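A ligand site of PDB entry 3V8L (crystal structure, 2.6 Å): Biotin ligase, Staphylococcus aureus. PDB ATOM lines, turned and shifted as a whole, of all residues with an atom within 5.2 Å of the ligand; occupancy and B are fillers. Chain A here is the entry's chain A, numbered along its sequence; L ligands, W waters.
The backbone carbonyl oxygen (O) of Met 143 sits at hydrogen-bond distance from the backbone NH (N) of Ile 215 (2.6 Å). The side-chain amide nitrogen (ND2) of Asn 218 lies close to the side-chain amide nitrogen (NE2) of Gln 221, 3.2 Å away. OE1 of Gln 122 sits at hydrogen-bond distance from N of Thr 100. The backbone carbonyl oxygen (O) of Ser 135 lies close to the indole nitrogen (NE1) of Trp 142. OG of Ser 135 sits at hydrogen-bond distance from NE2 of Gln 122, at 2.9 Å. N of Gly 214 sits at hydrogen-bond distance from O of Leu 198 (2.8 Å). The backbone carbonyl oxygen of Gly 125 sits at hydrogen-bond distance from the backbone NH of Trp 133 (2.9 Å). OE1 of Gln 101 lies within hydrogen-bond range of OG of Ser 144, at 2.6 Å.
Merely in contact with the ligand: Gly 127 (3.2 Å), Gly 196 (3.3 Å), Gly 125 (3.4 Å), Met 143 (3.4 Å), Ile 230 (3.5 Å), His 132 (3.5 Å), Trp 133 (3.5 Å), Ile 215 (3.6 Å), Gly 216 (3.7 Å), Asp 186 (3.7 Å), Gln 101 (3.7 Å), Ser 144 (3.8 Å), Gly 214 (3.8 Å), Phe 197 (3.9 Å), Ala 234 (3.9 Å) and Trp 142 (3.96 Å). Of the 33 residues printed, 25 come within 4 Å of the ligand. The nearest printed residue that does not touch the ligand is Asn 185 (4.04 Å).
Water W2 bridges O8 of the ligand and O of His 132. Water W3 lies within hydrogen-bond range of the side-chain amino group (NZ) of Lys 193 (3.0 Å), an oxygen (O4) of the ligand (3.4 Å) and the side-chain carboxylate (OD1) of Asp 186 (3.4 Å). Water W1 bridges the backbone carbonyl oxygen (O) of Arg 126 (3.1 Å) and an oxygen (O3) of the ligand (3.4 Å).
N of Arg 128 sits at hydrogen-bond distance from O5 of the ligand. The guanidinium group (NH1) of Arg 131 lies within salt-bridge range of an oxygen (O5) of the ligand (2.9 Å). OE1 of Gln 122 sits at hydrogen-bond distance from N1 of the ligand (3.1 Å). An oxygen (O3) of the ligand sits at hydrogen-bond distance from the backbone NH of Arg 126 (3.0 Å). The backbone carbonyl oxygen of Arg 128 lies close to an oxygen (O5) of the ligand (2.9 Å). NZ of Lys 193 is in salt-bridge range of O4 of the ligand (3.4 Å). OG of Ser 99 is in hydrogen-bond range of O3 of the ligand (2.7 Å). A nitrogen (N6) of the ligand lies close to the side-chain amide oxygen of Asn 218. The backbone carbonyl oxygen (O) of Ser 134 is in hydrogen-bond range of a nitrogen (N5) of the ligand (3.0 Å). The backbone carbonyl oxygen (O) of Arg 126 sits at hydrogen-bond distance from a nitrogen (N2) of the ligand. A nitrogen (N4) of the ligand sits at hydrogen-bond distance from the backbone NH of Ser 134, 3.1 Å away. OG1 of Thr 100 sits at hydrogen-bond distance from N1 of the ligand, at 3.3 Å.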
ATOM      1  N   SER A  99      -6.562  -8.212 -18.294  1.00  0.00           N
ATOM      2  CA  SER A  99      -7.102  -8.097 -19.616  1.00  0.00           C
ATOM      3  C   SER A  99      -7.584  -9.478 -20.038  1.00  0.00           C
ATOM      4  O   SER A  99      -6.880 -10.410 -19.819  1.00  0.00           O
ATOM      5  CB  SER A  99      -6.012  -7.574 -20.570  1.00  0.00           C
ATOM      6  OG  SER A  99      -6.347  -7.761 -21.940  1.00  0.00           O
ATOM      7  N   THR A 100      -8.784  -9.595 -20.643  1.00  0.00           N
ATOM      8  CA  THR A 100      -9.208 -10.887 -21.225  1.00  0.00           C
ATOM      9  C   THR A 100      -8.265 -11.342 -22.362  1.00  0.00           C
ATOM     10  O   THR A 100      -8.175 -12.545 -22.676  1.00  0.00           O
ATOM     11  CB  THR A 100     -10.622 -10.806 -21.828  1.00  0.00           C
ATOM     12  OG1 THR A 100     -10.622  -9.839 -22.880  1.00  0.00           O
ATOM     13  CG2 THR A 100     -11.749 -10.457 -20.789  1.00  0.00           C
ATOM     14  N   GLN A 101      -7.569 -10.395 -22.994  1.00  0.00           N
ATOM     15  CA  GLN A 101      -6.658 -10.696 -24.108  1.00  0.00           C
ATOM     16  C   GLN A 101      -5.390 -11.424 -23.643  1.00  0.00           C
ATOM     17  O   GLN A 101      -4.950 -12.393 -24.272  1.00  0.00           O
ATOM     18  CB  GLN A 101      -6.343  -9.422 -24.915  1.00  0.00           C
ATOM     19  CG  GLN A 101      -5.798  -9.745 -26.292  1.00  0.00           C
ATOM     20  CD  GLN A 101      -6.838 -10.128 -27.361  1.00  0.00           C
ATOM     21  OE1 GLN A 101      -8.008 -10.389 -27.082  1.00  0.00           O
ATOM     22  NE2 GLN A 101      -6.388 -10.148 -28.612  1.00  0.00           N
ATOM     23  N   GLN A 122     -11.834  -4.636 -16.692  1.00  0.00           N
ATOM     24  CA  GLN A 122     -10.391  -4.857 -16.931  1.00  0.00           C
ATOM     25  C   GLN A 122      -9.613  -3.703 -16.339  1.00  0.00           C
ATOM     26  O   GLN A 122     -10.018  -2.547 -16.518  1.00  0.00           O
ATOM     27  CB  GLN A 122     -10.054  -4.955 -18.424  1.00  0.00           C
ATOM     28  CG  GLN A 122     -10.930  -5.936 -19.178  1.00  0.00           C
ATOM     29  CD  GLN A 122     -10.543  -6.013 -20.663  1.00  0.00           C
ATOM     30  OE1 GLN A 122     -10.162  -7.072 -21.131  1.00  0.00           O
ATOM     31  NE2 GLN A 122     -10.651  -4.894 -21.378  1.00  0.00           N
ATOM     32  N   LYS A 124      -6.294  -3.356 -17.102  1.00  0.00           N
ATOM     33  CA  LYS A 124      -5.189  -3.101 -18.024  1.00  0.00           C
ATOM     34  C   LYS A 124      -5.660  -3.453 -19.451  1.00  0.00           C
ATOM     35  O   LYS A 124      -4.940  -4.183 -20.172  1.00  0.00           O
ATOM     36  CB  LYS A 124      -3.925  -3.886 -17.593  1.00  0.00           C
ATOM     37  CG  LYS A 124      -2.685  -3.434 -18.224  1.00  0.00           C
ATOM     38  CD  LYS A 124      -1.414  -4.051 -17.610  1.00  0.00           C
ATOM     39  CE  LYS A 124      -0.193  -3.261 -18.102  1.00  0.00           C
ATOM     40  NZ  LYS A 124       1.112  -3.864 -17.698  1.00  0.00           N
ATOM     41  N   GLY A 125      -6.854  -2.972 -19.814  1.00  0.00           N
ATOM     42  CA  GLY A 125      -7.381  -3.175 -21.169  1.00  0.00           C
ATOM     43  C   GLY A 125      -6.532  -2.373 -22.165  1.00  0.00           C
ATOM     44  O   GLY A 125      -6.228  -1.244 -21.895  1.00  0.00           O
ATOM     45  N   ARG A 126      -6.149  -2.999 -23.283  1.00  0.00           N
ATOM     46  CA  ARG A 126      -5.301  -2.380 -24.332  1.00  0.00           C
ATOM     47  C   ARG A 126      -5.991  -2.503 -25.709  1.00  0.00           C
ATOM     48  O   ARG A 126      -6.634  -3.516 -26.014  1.00  0.00           O
ATOM     49  CB  ARG A 126      -3.938  -3.069 -24.376  1.00  0.00           C
ATOM     50  CG  ARG A 126      -3.028  -2.807 -23.139  1.00  0.00           C
ATOM     51  CD  ARG A 126      -2.894  -1.294 -22.822  1.00  0.00           C
ATOM     52  NE  ARG A 126      -2.028  -0.958 -21.693  1.00  0.00           N
ATOM     53  CZ  ARG A 126      -2.457  -0.479 -20.508  1.00  0.00           C
ATOM     54  NH1 ARG A 126      -3.773  -0.292 -20.238  1.00  0.00           N
ATOM     55  NH2 ARG A 126      -1.577  -0.213 -19.580  1.00  0.00           N
ATOM     56  N   GLY A 127      -5.862  -1.492 -26.557  1.00  0.00           N
ATOM     57  CA  GLY A 127      -6.267  -1.645 -27.954  1.00  0.00           C
ATOM     58  C   GLY A 127      -5.065  -1.803 -28.873  1.00  0.00           C
ATOM     59  O   GLY A 127      -3.970  -2.225 -28.430  1.00  0.00           O
ATOM     60  N   ARG A 128      -5.250  -1.421 -30.143  1.00  0.00           N
ATOM     61  CA  ARG A 128      -4.160  -1.424 -31.115  1.00  0.00           C
ATOM     62  C   ARG A 128      -3.039  -0.550 -30.627  1.00  0.00           C
ATOM     63  O   ARG A 128      -3.230   0.434 -29.908  1.00  0.00           O
ATOM     64  CB  ARG A 128      -4.621  -0.978 -32.510  1.00  0.00           C
ATOM     65  CG  ARG A 128      -5.682  -1.880 -33.155  1.00  0.00           C
ATOM     66  CD  ARG A 128      -6.141  -1.233 -34.504  1.00  0.00           C
ATOM     67  NE  ARG A 128      -5.039  -1.107 -35.466  1.00  0.00           N
ATOM     68  CZ  ARG A 128      -5.068  -0.354 -36.568  1.00  0.00           C
ATOM     69  NH1 ARG A 128      -6.152   0.386 -36.814  1.00  0.00           N
ATOM     70  NH2 ARG A 128      -4.017  -0.320 -37.390  1.00  0.00           N
ATOM     71  N   PHE A 129      -1.827  -0.918 -31.008  1.00  0.00           N
ATOM     72  CA  PHE A 129      -0.654  -0.144 -30.643  1.00  0.00           C
ATOM     73  C   PHE A 129      -0.454  -0.036 -29.135  1.00  0.00           C
ATOM     74  O   PHE A 129       0.293   0.844 -28.680  1.00  0.00           O
ATOM     75  CB  PHE A 129      -0.652   1.252 -31.348  1.00  0.00           C
ATOM     76  CG  PHE A 129      -0.839   1.153 -32.833  1.00  0.00           C
ATOM     77  CD1 PHE A 129       0.210   0.728 -33.648  1.00  0.00           C
ATOM     78  CD2 PHE A 129      -2.051   1.476 -33.429  1.00  0.00           C
ATOM     79  CE1 PHE A 129       0.038   0.600 -35.035  1.00  0.00           C
ATOM     80  CE2 PHE A 129      -2.243   1.343 -34.829  1.00  0.00           C
ATOM     81  CZ  PHE A 129      -1.196   0.898 -35.618  1.00  0.00           C
ATOM     82  N   ARG A 131      -2.478   1.049 -26.943  1.00  0.00           N
ATOM     83  CA  ARG A 131      -3.255   2.143 -26.388  1.00  0.00           C
ATOM     84  C   ARG A 131      -4.208   1.664 -25.262  1.00  0.00           C
ATOM     85  O   ARG A 131      -4.772   0.579 -25.342  1.00  0.00           O
ATOM     86  CB  ARG A 131      -4.126   2.736 -27.487  1.00  0.00           C
ATOM     87  CG  ARG A 131      -3.395   3.613 -28.535  1.00  0.00           C
ATOM     88  CD  ARG A 131      -4.347   3.635 -29.719  1.00  0.00           C
ATOM     89  NE  ARG A 131      -3.737   4.320 -30.829  1.00  0.00           N
ATOM     90  CZ  ARG A 131      -4.071   4.195 -32.123  1.00  0.00           C
ATOM     91  NH1 ARG A 131      -5.050   3.382 -32.516  1.00  0.00           N
ATOM     92  NH2 ARG A 131      -3.391   4.902 -33.007  1.00  0.00           N
ATOM     93  N   HIS A 132      -4.410   2.500 -24.248  1.00  0.00           N
ATOM     94  CA  HIS A 132      -5.356   2.283 -23.154  1.00  0.00           C
ATOM     95  C   HIS A 132      -6.779   2.081 -23.700  1.00  0.00           C
ATOM     96  O   HIS A 132      -7.250   2.850 -24.538  1.00  0.00           O
ATOM     97  CB  HIS A 132      -5.284   3.486 -22.161  1.00  0.00           C
ATOM     98  CG  HIS A 132      -6.330   3.460 -21.091  1.00  0.00           C
ATOM     99  ND1 HIS A 132      -6.264   2.602 -20.000  1.00  0.00           N
ATOM    100  CD2 HIS A 132      -7.475   4.172 -20.935  1.00  0.00           C
ATOM    101  CE1 HIS A 132      -7.335   2.778 -19.244  1.00  0.00           C
ATOM    102  NE2 HIS A 132      -8.083   3.717 -19.782  1.00  0.00           N
ATOM    103  N   TRP A 133      -7.450   1.056 -23.228  1.00  0.00           N
ATOM    104  CA  TRP A 133      -8.836   0.813 -23.555  1.00  0.00           C
ATOM    105  C   TRP A 133      -9.608   0.848 -22.247  1.00  0.00           C
ATOM    106  O   TRP A 133      -9.366   0.048 -21.358  1.00  0.00           O
ATOM    107  CB  TRP A 133      -9.054  -0.535 -24.250  1.00  0.00           C
ATOM    108  CG  TRP A 133     -10.535  -0.752 -24.546  1.00  0.00           C
ATOM    109  CD1 TRP A 133     -11.462  -1.453 -23.778  1.00  0.00           C
ATOM    110  CD2 TRP A 133     -11.263  -0.212 -25.649  1.00  0.00           C
ATOM    111  NE1 TRP A 133     -12.716  -1.368 -24.350  1.00  0.00           N
ATOM    112  CE2 TRP A 133     -12.621  -0.636 -25.501  1.00  0.00           C
ATOM    113  CE3 TRP A 133     -10.912   0.589 -26.727  1.00  0.00           C
ATOM    114  CZ2 TRP A 133     -13.608  -0.268 -26.423  1.00  0.00           C
ATOM    115  CZ3 TRP A 133     -11.912   0.929 -27.656  1.00  0.00           C
ATOM    116  CH2 TRP A 133     -13.228   0.489 -27.500  1.00  0.00           C
ATOM    117  N   SER A 134     -10.505   1.815 -22.130  1.00  0.00           N
ATOM    118  CA  SER A 134     -11.312   1.996 -20.956  1.00  0.00           C
ATOM    119  C   SER A 134     -12.406   0.918 -20.841  1.00  0.00           C
ATOM    120  O   SER A 134     -13.180   0.708 -21.780  1.00  0.00           O
ATOM    121  CB  SER A 134     -11.878   3.410 -20.982  1.00  0.00           C
ATOM    122  OG  SER A 134     -12.649   3.635 -19.836  1.00  0.00           O
ATOM    123  N   SER A 135     -12.436   0.213 -19.700  1.00  0.00           N
ATOM    124  CA  SER A 135     -13.282  -0.972 -19.471  1.00  0.00           C
ATOM    125  C   SER A 135     -14.055  -0.957 -18.137  1.00  0.00           C
ATOM    126  O   SER A 135     -13.798  -1.799 -17.257  1.00  0.00           O
ATOM    127  CB  SER A 135     -12.399  -2.213 -19.436  1.00  0.00           C
ATOM    128  OG  SER A 135     -11.554  -2.290 -20.553  1.00  0.00           O
ATOM    129  N   LEU A 141     -19.154  -4.905 -22.810  1.00  0.00           N
ATOM    130  CA  LEU A 141     -18.805  -6.300 -23.050  1.00  0.00           C
ATOM    131  C   LEU A 141     -17.322  -6.295 -23.409  1.00  0.00           C
ATOM    132  O   LEU A 141     -16.930  -5.709 -24.432  1.00  0.00           O
ATOM    133  CB  LEU A 141     -19.661  -6.842 -24.195  1.00  0.00           C
ATOM    134  CG  LEU A 141     -19.384  -8.299 -24.617  1.00  0.00           C
ATOM    135  CD1 LEU A 141     -20.701  -9.023 -24.959  1.00  0.00           C
ATOM    136  CD2 LEU A 141     -18.450  -8.281 -25.820  1.00  0.00           C
ATOM    137  N   TRP A 142     -16.507  -6.909 -22.545  1.00  0.00           N
ATOM    138  CA  TRP A 142     -15.032  -7.013 -22.653  1.00  0.00           C
ATOM    139  C   TRP A 142     -14.710  -8.486 -22.778  1.00  0.00           C
ATOM    140  O   TRP A 142     -14.772  -9.211 -21.808  1.00  0.00           O
ATOM    141  CB  TRP A 142     -14.310  -6.378 -21.422  1.00  0.00           C
ATOM    142  CG  TRP A 142     -14.972  -5.126 -20.814  1.00  0.00           C
ATOM    143  CD1 TRP A 142     -15.300  -4.930 -19.493  1.00  0.00           C
ATOM    144  CD2 TRP A 142     -15.358  -3.895 -21.509  1.00  0.00           C
ATOM    145  NE1 TRP A 142     -15.891  -3.678 -19.322  1.00  0.00           N
ATOM    146  CE2 TRP A 142     -15.947  -3.036 -20.545  1.00  0.00           C
ATOM    147  CE3 TRP A 142     -15.271  -3.449 -22.840  1.00  0.00           C
ATOM    148  CZ2 TRP A 142     -16.422  -1.739 -20.871  1.00  0.00           C
ATOM    149  CZ3 TRP A 142     -15.773  -2.164 -23.181  1.00  0.00           C
ATOM    150  CH2 TRP A 142     -16.327  -1.332 -22.190  1.00  0.00           C
ATOM    151  N   MET A 143     -14.387  -8.909 -23.997  1.00  0.00           N
ATOM    152  CA  MET A 143     -14.348 -10.303 -24.369  1.00  0.00           C
ATOM    153  C   MET A 143     -13.152 -10.598 -25.289  1.00  0.00           C
ATOM    154  O   MET A 143     -12.801  -9.778 -26.136  1.00  0.00           O
ATOM    155  CB  MET A 143     -15.663 -10.681 -25.113  1.00  0.00           C
ATOM    156  CG  MET A 143     -15.806 -12.164 -25.403  1.00  0.00           C
ATOM    157  SD  MET A 143     -17.384 -12.707 -26.120  1.00  0.00           S
ATOM    158  CE  MET A 143     -17.476 -11.766 -27.605  1.00  0.00           C
ATOM    159  N   SER A 144     -12.554 -11.782 -25.124  1.00  0.00           N
ATOM    160  CA  SER A 144     -11.601 -12.330 -26.077  1.00  0.00           C
ATOM    161  C   SER A 144     -12.082 -13.702 -26.537  1.00  0.00           C
ATOM    162  O   SER A 144     -12.514 -14.558 -25.733  1.00  0.00           O
ATOM    163  CB  SER A 144     -10.172 -12.408 -25.482  1.00  0.00           C
ATOM    164  OG  SER A 144      -9.683 -11.074 -25.267  1.00  0.00           O
ATOM    165  N   ASN A 185     -10.913  -1.656 -37.806  1.00  0.00           N
ATOM    166  CA  ASN A 185     -11.088  -2.157 -36.432  1.00  0.00           C
ATOM    167  C   ASN A 185     -12.091  -1.470 -35.492  1.00  0.00           C
ATOM    168  O   ASN A 185     -12.012  -1.646 -34.273  1.00  0.00           O
ATOM    169  CB  ASN A 185      -9.722  -2.082 -35.754  1.00  0.00           C
ATOM    170  CG  ASN A 185      -8.828  -3.259 -36.126  1.00  0.00           C
ATOM    171  OD1 ASN A 185      -7.794  -3.089 -36.814  1.00  0.00           O
ATOM    172  ND2 ASN A 185      -9.219  -4.479 -35.692  1.00  0.00           N
ATOM    173  N   ASP A 186     -12.960  -0.603 -36.013  1.00  0.00           N
ATOM    174  CA  ASP A 186     -13.859   0.181 -35.168  1.00  0.00           C
ATOM    175  C   ASP A 186     -15.293   0.074 -35.651  1.00  0.00           C
ATOM    176  O   ASP A 186     -15.541  -0.109 -36.840  1.00  0.00           O
ATOM    177  CB  ASP A 186     -13.478   1.672 -35.169  1.00  0.00           C
ATOM    178  CG  ASP A 186     -12.067   1.928 -34.673  1.00  0.00           C
ATOM    179  OD1 ASP A 186     -11.638   3.079 -34.710  1.00  0.00           O
ATOM    180  OD2 ASP A 186     -11.370   1.024 -34.233  1.00  0.00           O
ATOM    181  N   LYS A 193     -17.707   6.164 -31.533  1.00  0.00           N
ATOM    182  CA  LYS A 193     -17.184   4.789 -31.490  1.00  0.00           C
ATOM    183  C   LYS A 193     -17.897   3.941 -30.403  1.00  0.00           C
ATOM    184  O   LYS A 193     -17.826   4.248 -29.238  1.00  0.00           O
ATOM    185  CB  LYS A 193     -15.653   4.810 -31.287  1.00  0.00           C
ATOM    186  CG  LYS A 193     -14.959   3.450 -31.384  1.00  0.00           C
ATOM    187  CD  LYS A 193     -13.452   3.590 -31.259  1.00  0.00           C
ATOM    188  CE  LYS A 193     -12.809   2.263 -31.002  1.00  0.00           C
ATOM    189  NZ  LYS A 193     -11.314   2.362 -31.236  1.00  0.00           N
ATOM    190  N   GLY A 196     -14.387  -1.313 -30.333  1.00  0.00           N
ATOM    191  CA  GLY A 196     -13.116  -1.602 -30.989  1.00  0.00           C
ATOM    192  C   GLY A 196     -12.839  -3.090 -30.864  1.00  0.00           C
ATOM    193  O   GLY A 196     -13.166  -3.723 -29.848  1.00  0.00           O
ATOM    194  N   PHE A 197     -12.263  -3.672 -31.899  1.00  0.00           N
ATOM    195  CA  PHE A 197     -11.912  -5.072 -31.831  1.00  0.00           C
ATOM    196  C   PHE A 197     -10.499  -5.163 -32.412  1.00  0.00           C
ATOM    197  O   PHE A 197     -10.123  -4.338 -33.216  1.00  0.00           O
ATOM    198  CB  PHE A 197     -12.940  -5.999 -32.551  1.00  0.00           C
ATOM    199  CG  PHE A 197     -13.162  -5.656 -34.007  1.00  0.00           C
ATOM    200  CD1 PHE A 197     -14.084  -4.649 -34.386  1.00  0.00           C
ATOM    201  CD2 PHE A 197     -12.424  -6.305 -35.016  1.00  0.00           C
ATOM    202  CE1 PHE A 197     -14.242  -4.302 -35.724  1.00  0.00           C
ATOM    203  CE2 PHE A 197     -12.588  -5.961 -36.376  1.00  0.00           C
ATOM    204  CZ  PHE A 197     -13.492  -4.955 -36.714  1.00  0.00           C
ATOM    205  N   LEU A 198      -9.777  -6.198 -32.000  1.00  0.00           N
ATOM    206  CA  LEU A 198      -8.357  -6.381 -32.243  1.00  0.00           C
ATOM    207  C   LEU A 198      -8.165  -7.902 -32.552  1.00  0.00           C
ATOM    208  O   LEU A 198      -8.417  -8.724 -31.688  1.00  0.00           O
ATOM    209  CB  LEU A 198      -7.637  -6.011 -30.931  1.00  0.00           C
ATOM    210  CG  LEU A 198      -6.159  -6.210 -30.628  1.00  0.00           C
ATOM    211  CD1 LEU A 198      -5.272  -5.322 -31.458  1.00  0.00           C
ATOM    212  CD2 LEU A 198      -5.958  -5.882 -29.193  1.00  0.00           C
ATOM    213  N   GLY A 214      -9.996  -9.872 -29.645  1.00  0.00           N
ATOM    214  CA  GLY A 214     -10.403  -9.070 -28.508  1.00  0.00           C
ATOM    215  C   GLY A 214     -11.509  -8.097 -28.886  1.00  0.00           C
ATOM    216  O   GLY A 214     -11.354  -7.315 -29.775  1.00  0.00           O
ATOM    217  N   ILE A 215     -12.643  -8.151 -28.208  1.00  0.00           N
ATOM    218  CA  ILE A 215     -13.788  -7.346 -28.617  1.00  0.00           C
ATOM    219  C   ILE A 215     -14.327  -6.531 -27.423  1.00  0.00           C
ATOM    220  O   ILE A 215     -14.698  -7.107 -26.407  1.00  0.00           O
ATOM    221  CB  ILE A 215     -14.926  -8.212 -29.175  1.00  0.00           C
ATOM    222  CG1 ILE A 215     -14.472  -9.074 -30.364  1.00  0.00           C
ATOM    223  CG2 ILE A 215     -16.205  -7.328 -29.595  1.00  0.00           C
ATOM    224  CD1 ILE A 215     -15.471 -10.176 -30.732  1.00  0.00           C
ATOM    225  N   GLY A 216     -14.360  -5.206 -27.571  1.00  0.00           N
ATOM    226  CA  GLY A 216     -14.826  -4.320 -26.521  1.00  0.00           C
ATOM    227  C   GLY A 216     -15.963  -3.483 -27.066  1.00  0.00           C
ATOM    228  O   GLY A 216     -15.776  -2.717 -28.008  1.00  0.00           O
ATOM    229  N   ASN A 218     -19.160  -0.915 -25.929  1.00  0.00           N
ATOM    230  CA  ASN A 218     -19.786  -0.059 -24.926  1.00  0.00           C
ATOM    231  C   ASN A 218     -21.302  -0.308 -24.892  1.00  0.00           C
ATOM    232  O   ASN A 218     -22.000  -0.094 -25.873  1.00  0.00           O
ATOM    233  CB  ASN A 218     -19.478   1.402 -25.217  1.00  0.00           C
ATOM    234  CG  ASN A 218     -17.979   1.734 -25.232  1.00  0.00           C
ATOM    235  OD1 ASN A 218     -17.530   2.510 -26.064  1.00  0.00           O
ATOM    236  ND2 ASN A 218     -17.225   1.206 -24.301  1.00  0.00           N
ATOM    237  N   GLN A 221     -22.962   2.887 -20.883  1.00  0.00           N
ATOM    238  CA  GLN A 221     -22.504   4.233 -20.502  1.00  0.00           C
ATOM    239  C   GLN A 221     -23.499   5.336 -20.864  1.00  0.00           C
ATOM    240  O   GLN A 221     -24.087   5.336 -21.969  1.00  0.00           O
ATOM    241  CB  GLN A 221     -21.156   4.584 -21.150  1.00  0.00           C
ATOM    242  CG  GLN A 221     -20.015   3.781 -20.689  1.00  0.00           C
ATOM    243  CD  GLN A 221     -19.812   2.508 -21.537  1.00  0.00           C
ATOM    244  OE1 GLN A 221     -20.758   2.004 -22.164  1.00  0.00           O
ATOM    245  NE2 GLN A 221     -18.587   2.004 -21.547  1.00  0.00           N
ATOM    246  N   PHE A 226     -18.129   8.546 -19.738  1.00  0.00           N
ATOM    247  CA  PHE A 226     -17.033   8.380 -20.665  1.00  0.00           C
ATOM    248  C   PHE A 226     -15.739   9.137 -20.307  1.00  0.00           C
ATOM    249  O   PHE A 226     -14.658   8.756 -20.740  1.00  0.00           O
ATOM    250  CB  PHE A 226     -17.482   8.669 -22.096  1.00  0.00           C
ATOM    251  CG  PHE A 226     -18.020   7.464 -22.789  1.00  0.00           C
ATOM    252  CD1 PHE A 226     -17.216   6.356 -22.995  1.00  0.00           C
ATOM    253  CD2 PHE A 226     -19.339   7.427 -23.218  1.00  0.00           C
ATOM    254  CE1 PHE A 226     -17.695   5.245 -23.611  1.00  0.00           C
ATOM    255  CE2 PHE A 226     -19.825   6.311 -23.846  1.00  0.00           C
ATOM    256  CZ  PHE A 226     -19.000   5.222 -24.036  1.00  0.00           C
ATOM    257  N   ILE A 230     -12.512  11.543 -24.610  1.00  0.00           N
ATOM    258  CA  ILE A 230     -13.012  10.576 -25.605  1.00  0.00           C
ATOM    259  C   ILE A 230     -14.533  10.825 -25.786  1.00  0.00           C
ATOM    260  O   ILE A 230     -15.094  10.474 -26.816  1.00  0.00           O
ATOM    261  CB  ILE A 230     -12.666   9.046 -25.321  1.00  0.00           C
ATOM    262  CG1 ILE A 230     -13.167   8.566 -23.951  1.00  0.00           C
ATOM    263  CG2 ILE A 230     -11.152   8.728 -25.568  1.00  0.00           C
ATOM    264  CD1 ILE A 230     -13.392   7.091 -23.844  1.00  0.00           C
ATOM    265  N   ALA A 234     -17.123   8.995 -28.405  1.00  0.00           N
ATOM    266  CA  ALA A 234     -17.484   7.686 -27.866  1.00  0.00           C
ATOM    267  C   ALA A 234     -18.998   7.555 -27.651  1.00  0.00           C
ATOM    268  O   ALA A 234     -19.687   8.522 -27.356  1.00  0.00           O
ATOM    269  CB  ALA A 234     -16.737   7.439 -26.551  1.00  0.00           C
HETATM  270  C1  LIG L   1      -9.161  -0.881 -30.465  1.00  0.00           C
HETATM  271  O1  LIG L   1      -7.813  -0.330 -30.470  1.00  0.00           O
HETATM  272  O2  LIG L   1     -10.067  -0.239 -31.020  1.00  0.00           O
HETATM  273  C2  LIG L   1      -9.526  -1.969 -29.783  1.00  0.00           C
HETATM  274  C3  LIG L   1      -9.723  -2.448 -28.508  1.00  0.00           C
HETATM  275  C4  LIG L   1      -9.987  -3.876 -28.134  1.00  0.00           C
HETATM  276  C5  LIG L   1     -10.580  -3.843 -26.734  1.00  0.00           C
HETATM  277  C6  LIG L   1     -10.926  -5.252 -26.197  1.00  0.00           C
HETATM  278  S1  LIG L   1     -11.799  -5.191 -24.633  1.00  0.00           S
HETATM  279  C7  LIG L   1     -11.547  -6.967 -24.617  1.00  0.00           C
HETATM  280  C8  LIG L   1     -10.123  -7.296 -25.109  1.00  0.00           C
HETATM  281  N1  LIG L   1      -9.159  -7.154 -24.040  1.00  0.00           N
HETATM  282  C9  LIG L   1      -8.300  -6.121 -24.241  1.00  0.00           C
HETATM  283  O3  LIG L   1      -7.464  -5.739 -23.412  1.00  0.00           O
HETATM  284  N2  LIG L   1      -8.521  -5.574 -25.414  1.00  0.00           N
HETATM  285  C10 LIG L   1      -9.682  -6.209 -26.095  1.00  0.00           C
HETATM  286  P1  LIG L   1      -7.377   1.256 -30.786  1.00  0.00           P
HETATM  287  O4  LIG L   1      -8.056   1.871 -32.022  1.00  0.00           O
HETATM  288  O5  LIG L   1      -5.858   1.145 -30.924  1.00  0.00           O
HETATM  289  O6  LIG L   1      -7.460   2.221 -29.437  1.00  0.00           O
HETATM  290  C11 LIG L   1      -8.592   2.592 -28.650  1.00  0.00           C
HETATM  291  C12 LIG L   1      -8.830   4.089 -28.842  1.00  0.00           C
HETATM  292  O7  LIG L   1     -10.237   4.394 -28.715  1.00  0.00           O
HETATM  293  C13 LIG L   1      -8.116   4.882 -27.731  1.00  0.00           C
HETATM  294  O8  LIG L   1      -6.837   5.465 -28.103  1.00  0.00           O
HETATM  295  C14 LIG L   1      -9.138   5.911 -27.206  1.00  0.00           C
HETATM  296  O9  LIG L   1      -9.095   7.184 -27.876  1.00  0.00           O
HETATM  297  C15 LIG L   1     -10.469   5.262 -27.562  1.00  0.00           C
HETATM  298  N3  LIG L   1     -11.053   4.510 -26.404  1.00  0.00           N
HETATM  299  C16 LIG L   1     -10.489   4.026 -25.278  1.00  0.00           C
HETATM  300  N4  LIG L   1     -11.458   3.419 -24.543  1.00  0.00           N
HETATM  301  C17 LIG L   1     -12.641   3.511 -25.232  1.00  0.00           C
HETATM  302  C18 LIG L   1     -13.968   3.078 -25.013  1.00  0.00           C
HETATM  303  N5  LIG L   1     -14.379   2.387 -23.913  1.00  0.00           N
HETATM  304  N6  LIG L   1     -14.925   3.359 -25.933  1.00  0.00           N
HETATM  305  C19 LIG L   1     -14.726   4.098 -27.169  1.00  0.00           C
HETATM  306  N7  LIG L   1     -13.339   4.511 -27.327  1.00  0.00           N
HETATM  307  C20 LIG L   1     -12.368   4.214 -26.400  1.00  0.00           C
HETATM  308  O   HOH W   1      -5.131  -6.211 -25.897  1.00  0.00           O
HETATM  309  O   HOH W   2      -6.604   5.357 -25.430  1.00  0.00           O
HETATM  310  O   HOH W   3      -9.809   4.717 -32.346  1.00  0.00           O
